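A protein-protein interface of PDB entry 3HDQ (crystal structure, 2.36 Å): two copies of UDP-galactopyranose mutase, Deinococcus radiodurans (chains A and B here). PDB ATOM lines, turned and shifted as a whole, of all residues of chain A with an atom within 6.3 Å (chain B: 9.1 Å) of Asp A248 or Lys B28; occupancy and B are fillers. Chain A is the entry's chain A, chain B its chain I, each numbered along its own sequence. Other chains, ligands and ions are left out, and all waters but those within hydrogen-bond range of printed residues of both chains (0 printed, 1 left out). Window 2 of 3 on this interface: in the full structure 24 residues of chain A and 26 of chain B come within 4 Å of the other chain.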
ATOM      1  N   TYR A 243     -16.583   6.626  12.536  1.00  0.00           N
ATOM      2  CA  TYR A 243     -16.173   7.508  11.441  1.00  0.00           C
ATOM      3  C   TYR A 243     -14.947   8.313  11.839  1.00  0.00           C
ATOM      4  O   TYR A 243     -14.091   8.624  11.006  1.00  0.00           O
ATOM      5  CB  TYR A 243     -17.298   8.439  10.979  1.00  0.00           C
ATOM      6  CG  TYR A 243     -17.555   9.619  11.896  1.00  0.00           C
ATOM      7  CD1 TYR A 243     -17.097  10.890  11.579  1.00  0.00           C
ATOM      8  CD2 TYR A 243     -18.268   9.457  13.075  1.00  0.00           C
ATOM      9  CE1 TYR A 243     -17.338  11.975  12.429  1.00  0.00           C
ATOM     10  CE2 TYR A 243     -18.517  10.521  13.924  1.00  0.00           C
ATOM     11  CZ  TYR A 243     -18.048  11.778  13.601  1.00  0.00           C
ATOM     12  OH  TYR A 243     -18.302  12.827  14.456  1.00  0.00           O
ATOM     13  N   ARG A 244     -14.849   8.629  13.120  1.00  0.00           N
ATOM     14  CA  ARG A 244     -13.723   9.413  13.598  1.00  0.00           C
ATOM     15  C   ARG A 244     -12.371   8.710  13.442  1.00  0.00           C
ATOM     16  O   ARG A 244     -11.352   9.367  13.277  1.00  0.00           O
ATOM     17  CB  ARG A 244     -13.963   9.868  15.034  1.00  0.00           C
ATOM     18  CG  ARG A 244     -15.139  10.834  15.130  1.00  0.00           C
ATOM     19  CD  ARG A 244     -15.382  11.294  16.555  1.00  0.00           C
ATOM     20  NE  ARG A 244     -15.894  10.223  17.406  1.00  0.00           N
ATOM     21  CZ  ARG A 244     -17.090  10.234  17.987  1.00  0.00           C
ATOM     22  NH1 ARG A 244     -17.905  11.273  17.812  1.00  0.00           N
ATOM     23  NH2 ARG A 244     -17.467   9.212  18.751  1.00  0.00           N
ATOM     24  N   GLU A 245     -12.354   7.381  13.468  1.00  0.00           N
ATOM     25  CA  GLU A 245     -11.103   6.658  13.238  1.00  0.00           C
ATOM     26  C   GLU A 245     -10.644   6.779  11.781  1.00  0.00           C
ATOM     27  O   GLU A 245      -9.538   6.371  11.443  1.00  0.00           O
ATOM     28  CB  GLU A 245     -11.229   5.184  13.621  1.00  0.00           C
ATOM     29  CG  GLU A 245     -11.722   4.932  15.040  1.00  0.00           C
ATOM     30  CD  GLU A 245     -11.969   3.458  15.309  1.00  0.00           C
ATOM     31  OE1 GLU A 245     -13.140   3.024  15.277  1.00  0.00           O
ATOM     32  OE2 GLU A 245     -10.987   2.724  15.520  1.00  0.00           O
ATOM     33  N   ILE A 246     -11.478   7.390  10.941  1.00  0.00           N
ATOM     34  CA  ILE A 246     -11.291   7.328   9.493  1.00  0.00           C
ATOM     35  C   ILE A 246     -11.292   8.700   8.809  1.00  0.00           C
ATOM     36  O   ILE A 246     -10.650   8.891   7.775  1.00  0.00           O
ATOM     37  CB  ILE A 246     -12.370   6.403   8.871  1.00  0.00           C
ATOM     38  CG1 ILE A 246     -11.704   5.210   8.210  1.00  0.00           C
ATOM     39  CG2 ILE A 246     -13.344   7.151   7.957  1.00  0.00           C
ATOM     40  CD1 ILE A 246     -10.867   4.440   9.184  1.00  0.00           C
ATOM     41  N   ALA A 247     -11.994   9.655   9.411  1.00  0.00           N
ATOM     42  CA  ALA A 247     -12.255  10.959   8.793  1.00  0.00           C
ATOM     43  C   ALA A 247     -11.038  11.870   8.556  1.00  0.00           C
ATOM     44  O   ALA A 247     -11.119  12.815   7.784  1.00  0.00           O
ATOM     45  CB  ALA A 247     -13.324  11.707   9.583  1.00  0.00           C
ATOM     46  N   ASP A 248      -9.917  11.592   9.209  1.00  0.00           N
ATOM     47  CA  ASP A 248      -8.724  12.404   9.008  1.00  0.00           C
ATOM     48  C   ASP A 248      -7.996  12.074   7.716  1.00  0.00           C
ATOM     49  O   ASP A 248      -7.302  12.924   7.162  1.00  0.00           O
ATOM     50  CB  ASP A 248      -7.759  12.249  10.183  1.00  0.00           C
ATOM     51  CG  ASP A 248      -8.232  12.977  11.413  1.00  0.00           C
ATOM     52  OD1 ASP A 248      -9.158  13.806  11.274  1.00  0.00           O
ATOM     53  OD2 ASP A 248      -7.681  12.725  12.509  1.00  0.00           O
ATOM     54  N   PHE A 249      -8.142  10.846   7.231  1.00  0.00           N
ATOM     55  CA  PHE A 249      -7.350  10.428   6.078  1.00  0.00           C
ATOM     56  C   PHE A 249      -8.126   9.906   4.868  1.00  0.00           C
ATOM     57  O   PHE A 249      -7.603   9.894   3.762  1.00  0.00           O
ATOM     58  CB  PHE A 249      -6.242   9.447   6.488  1.00  0.00           C
ATOM     59  CG  PHE A 249      -6.744   8.185   7.133  1.00  0.00           C
ATOM     60  CD1 PHE A 249      -6.751   8.051   8.513  1.00  0.00           C
ATOM     61  CD2 PHE A 249      -7.182   7.121   6.358  1.00  0.00           C
ATOM     62  CE1 PHE A 249      -7.200   6.879   9.112  1.00  0.00           C
ATOM     63  CE2 PHE A 249      -7.629   5.952   6.944  1.00  0.00           C
ATOM     64  CZ  PHE A 249      -7.639   5.831   8.325  1.00  0.00           C
ATOM     65  N   ILE A 250      -9.364   9.476   5.051  1.00  0.00           N
ATOM     66  CA  ILE A 250     -10.123   9.051   3.886  1.00  0.00           C
ATOM     67  C   ILE A 250     -10.839  10.246   3.281  1.00  0.00           C
ATOM     68  O   ILE A 250     -11.678  10.857   3.930  1.00  0.00           O
ATOM     69  CB  ILE A 250     -11.142   7.942   4.203  1.00  0.00           C
ATOM     70  CG1 ILE A 250     -10.441   6.659   4.637  1.00  0.00           C
ATOM     71  CG2 ILE A 250     -11.992   7.650   2.978  1.00  0.00           C
ATOM     72  CD1 ILE A 250     -11.402   5.503   4.842  1.00  0.00           C
ATOM     73  N   PHE A 252     -13.453  12.485   1.400  1.00  0.00           N
ATOM     74  CA  PHE A 252     -14.867  12.520   1.037  1.00  0.00           C
ATOM     75  C   PHE A 252     -15.339  13.954   0.788  1.00  0.00           C
ATOM     76  O   PHE A 252     -14.855  14.883   1.418  1.00  0.00           O
ATOM     77  CB  PHE A 252     -15.733  11.867   2.126  1.00  0.00           C
ATOM     78  CG  PHE A 252     -15.633  12.534   3.476  1.00  0.00           C
ATOM     79  CD1 PHE A 252     -16.553  13.498   3.857  1.00  0.00           C
ATOM     80  CD2 PHE A 252     -14.624  12.189   4.365  1.00  0.00           C
ATOM     81  CE1 PHE A 252     -16.473  14.109   5.114  1.00  0.00           C
ATOM     82  CE2 PHE A 252     -14.530  12.788   5.622  1.00  0.00           C
ATOM     83  CZ  PHE A 252     -15.460  13.754   5.999  1.00  0.00           C
ATOM     84  N   SER B  27      -6.461   8.209  14.755  1.00  0.00           N
ATOM     85  CA  SER B  27      -5.592   7.423  13.879  1.00  0.00           C
ATOM     86  C   SER B  27      -5.342   8.154  12.559  1.00  0.00           C
ATOM     87  O   SER B  27      -6.195   8.919  12.089  1.00  0.00           O
ATOM     88  CB  SER B  27      -6.194   6.037  13.619  1.00  0.00           C
ATOM     89  OG  SER B  27      -5.399   5.286  12.711  1.00  0.00           O
ATOM     90  N   LYS B  28      -4.175   7.916  11.960  1.00  0.00           N
ATOM     91  CA  LYS B  28      -3.793   8.623  10.739  1.00  0.00           C
ATOM     92  C   LYS B  28      -3.575   7.692   9.549  1.00  0.00           C
ATOM     93  O   LYS B  28      -3.257   8.150   8.441  1.00  0.00           O
ATOM     94  CB  LYS B  28      -2.543   9.468  10.976  1.00  0.00           C
ATOM     95  CG  LYS B  28      -2.571  10.803  10.242  1.00  0.00           C
ATOM     96  CD  LYS B  28      -3.718  11.669  10.742  1.00  0.00           C
ATOM     97  CE  LYS B  28      -3.697  11.774  12.265  1.00  0.00           C
ATOM     98  NZ  LYS B  28      -4.794  12.630  12.796  1.00  0.00           N
ATOM     99  N   GLY B  29      -3.752   6.392   9.786  1.00  0.00           N
ATOM    100  CA  GLY B  29      -3.597   5.389   8.747  1.00  0.00           C
ATOM    101  C   GLY B  29      -3.569   3.973   9.288  1.00  0.00           C
ATOM    102  O   GLY B  29      -3.973   3.723  10.425  1.00  0.00           O
ATOM    103  N   PHE B  30      -3.078   3.046   8.468  1.00  0.00           N
ATOM    104  CA  PHE B  30      -3.077   1.624   8.802  1.00  0.00           C
ATOM    105  C   PHE B  30      -1.680   1.020   8.663  1.00  0.00           C
ATOM    106  O   PHE B  30      -0.943   1.349   7.737  1.00  0.00           O
ATOM    107  CB  PHE B  30      -4.036   0.849   7.880  1.00  0.00           C
ATOM    108  CG  PHE B  30      -5.493   1.171   8.090  1.00  0.00           C
ATOM    109  CD1 PHE B  30      -6.157   2.015   7.221  1.00  0.00           C
ATOM    110  CD2 PHE B  30      -6.193   0.621   9.152  1.00  0.00           C
ATOM    111  CE1 PHE B  30      -7.489   2.315   7.404  1.00  0.00           C
ATOM    112  CE2 PHE B  30      -7.531   0.916   9.349  1.00  0.00           C
ATOM    113  CZ  PHE B  30      -8.181   1.767   8.471  1.00  0.00           C
ATOM    114  N   ASP B  31      -1.333   0.114   9.569  1.00  0.00           N
ATOM    115  CA  ASP B  31      -0.114  -0.667   9.430  1.00  0.00           C
ATOM    116  C   ASP B  31      -0.197  -1.692   8.272  1.00  0.00           C
ATOM    117  O   ASP B  31       0.774  -1.883   7.530  1.00  0.00           O
ATOM    118  CB  ASP B  31       0.223  -1.335  10.764  1.00  0.00           C
ATOM    119  CG  ASP B  31       0.518  -0.318  11.865  1.00  0.00           C
ATOM    120  OD1 ASP B  31       1.453   0.492  11.676  1.00  0.00           O
ATOM    121  OD2 ASP B  31      -0.178  -0.320  12.909  1.00  0.00           O
ATOM    122  N   ARG B  54      -2.530  -1.742  13.458  1.00  0.00           N
ATOM    123  CA  ARG B  54      -3.773  -1.262  12.848  1.00  0.00           C
ATOM    124  C   ARG B  54      -3.971  -1.934  11.494  1.00  0.00           C
ATOM    125  O   ARG B  54      -3.146  -1.790  10.585  1.00  0.00           O
ATOM    126  CB  ARG B  54      -3.770   0.260  12.674  1.00  0.00           C
ATOM    127  CG  ARG B  54      -3.641   1.067  13.956  1.00  0.00           C
ATOM    128  CD  ARG B  54      -4.863   0.920  14.877  1.00  0.00           C
ATOM    129  NE  ARG B  54      -6.039   1.683  14.444  1.00  0.00           N
ATOM    130  CZ  ARG B  54      -7.190   1.718  15.116  1.00  0.00           C
ATOM    131  NH1 ARG B  54      -7.317   1.037  16.250  1.00  0.00           N
ATOM    132  NH2 ARG B  54      -8.212   2.431  14.657  1.00  0.00           N
ATOM    133  N   PHE B 249      -5.653   5.957  -2.059  1.00  0.00           N
ATOM    134  CA  PHE B 249      -5.876   7.040  -1.097  1.00  0.00           C
ATOM    135  C   PHE B 249      -6.095   6.642   0.366  1.00  0.00           C
ATOM    136  O   PHE B 249      -6.536   7.459   1.174  1.00  0.00           O
ATOM    137  CB  PHE B 249      -7.002   7.969  -1.572  1.00  0.00           C
ATOM    138  CG  PHE B 249      -8.331   7.287  -1.743  1.00  0.00           C
ATOM    139  CD1 PHE B 249      -8.970   7.290  -2.971  1.00  0.00           C
ATOM    140  CD2 PHE B 249      -8.943   6.653  -0.676  1.00  0.00           C
ATOM    141  CE1 PHE B 249     -10.194   6.673  -3.130  1.00  0.00           C
ATOM    142  CE2 PHE B 249     -10.167   6.030  -0.830  1.00  0.00           C
ATOM    143  CZ  PHE B 249     -10.795   6.040  -2.055  1.00  0.00           C
ATOM    144  N   ILE B 250      -5.788   5.401   0.712  1.00  0.00           N
ATOM    145  CA  ILE B 250      -5.726   5.032   2.118  1.00  0.00           C
ATOM    146  C   ILE B 250      -4.278   4.700   2.487  1.00  0.00           C
ATOM    147  O   ILE B 250      -3.621   3.931   1.789  1.00  0.00           O
ATOM    148  CB  ILE B 250      -6.675   3.862   2.446  1.00  0.00           C
ATOM    149  CG1 ILE B 250      -8.133   4.307   2.275  1.00  0.00           C
ATOM    150  CG2 ILE B 250      -6.417   3.357   3.852  1.00  0.00           C
ATOM    151  CD1 ILE B 250      -9.161   3.291   2.744  1.00  0.00           C
ATOM    152  N   PRO B 251      -3.764   5.311   3.566  1.00  0.00           N
ATOM    153  CA  PRO B 251      -2.369   5.118   3.969  1.00  0.00           C
ATOM    154  C   PRO B 251      -2.161   3.759   4.586  1.00  0.00           C
ATOM    155  O   PRO B 251      -2.899   3.406   5.500  1.00  0.00           O
ATOM    156  CB  PRO B 251      -2.150   6.191   5.053  1.00  0.00           C
ATOM    157  CG  PRO B 251      -3.303   7.136   4.922  1.00  0.00           C
ATOM    158  CD  PRO B 251      -4.447   6.306   4.407  1.00  0.00           C
ATOM    159  N   PHE B 252      -1.162   3.021   4.108  1.00  0.00           N
ATOM    160  CA  PHE B 252      -0.785   1.752   4.713  1.00  0.00           C
ATOM    161  C   PHE B 252       0.669   1.405   4.416  1.00  0.00           C
ATOM    162  O   PHE B 252       1.168   1.688   3.329  1.00  0.00           O
ATOM    163  CB  PHE B 252      -1.713   0.632   4.235  1.00  0.00           C
ATOM    164  CG  PHE B 252      -1.610   0.334   2.772  1.00  0.00           C
ATOM    165  CD1 PHE B 252      -0.787  -0.677   2.319  1.00  0.00           C
ATOM    166  CD2 PHE B 252      -2.350   1.046   1.850  1.00  0.00           C
ATOM    167  CE1 PHE B 252      -0.697  -0.968   0.979  1.00  0.00           C
ATOM    168  CE2 PHE B 252      -2.263   0.760   0.499  1.00  0.00           C
ATOM    169  CZ  PHE B 252      -1.432  -0.253   0.069  1.00  0.00           C
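The guanidinium group (NH2) of Arg B54 lies within salt-bridge range of the side-chain carboxylate (OE2) of Glu A245 (2.9 Å). NZ of Lys B28 lies within salt-bridge range of OD2 of Asp A248.
The backbone NH (N) of Phe B30 sits at hydrogen-bond distance from the backbone carbonyl oxygen (O) of Pro B251, 3.0 Å away. N of Arg B54 is in hydrogen-bond range of OD2 of Asp B31 (2.8 Å). The side-chain hydroxyl (OG) of Ser B27 is in hydrogen-bond range of the backbone carbonyl oxygen (O) of Gly B29, at 3.1 Å.
CD1 of Ile A246 touches CZ of Phe B30 (3.9 Å). CD1 of Phe A249 touches O of Ser B27, 3.7 Å away. Phe A249 touches Lys B28. CE1 of Phe A249 touches N of Gly B29, at 3.5 Å. Phe B30 touches Phe A249 (CE1 to CZ, 3.6 Å). Phe A249 touches Phe B249. Pro B251 touches Phe A249 (CD to CD2, 3.5 Å). CD1 of Ile B250 touches CD1 of Ile A250, at 3.8 Å.
Asp A248 touches just one residue of chain B: Lys B28 (2.9 Å). Of chain A, only Asp A248 (2.9 Å) and Phe A249 (3.4 Å) come within 4 Å of Lys B28. Of the printed residues of chain A, Phe B249 touches Phe A249. Of the printed residues of chain B, Ile A250 touches Ile B250. Of the printed residues of chain B, Ile A246 touches Phe B30. Printed residues of chain B within 4 Å of Phe A249: Ser B27, Lys B28, Gly B29, Phe B30, Phe B249 and Pro B251. Of the printed residues of chain B, Glu A245 touches Arg B54 (2.9 Å). Phe A252 touches none of the printed residues of chain B.
Hydrophobic or aromatic side chains of chain B that line the printed part of chain A: Phe B30, Ile B250 and Pro B251. Of the 9 printed residues of chain A, 5 touch a printed residue of chain B. Hydrophobic or aromatic side chains of chain A within 4 Å of the printed part of chain B: Ile A246, Phe A249 and Ile A250. Among the printed residues, 10 pairs touch across the chains. Among the printed residues, Asp or Glu carboxylates within 4 Å of a Lys or Arg side-chain nitrogen of the other chain: Glu A245 with Arg B54 (2.9 Å) and Asp A248 with Lys B28 (2.9 Å).
Phe B249 touches its own counterpart, Phe A249. Ile A250 touches its own counterpart, Ile B250.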
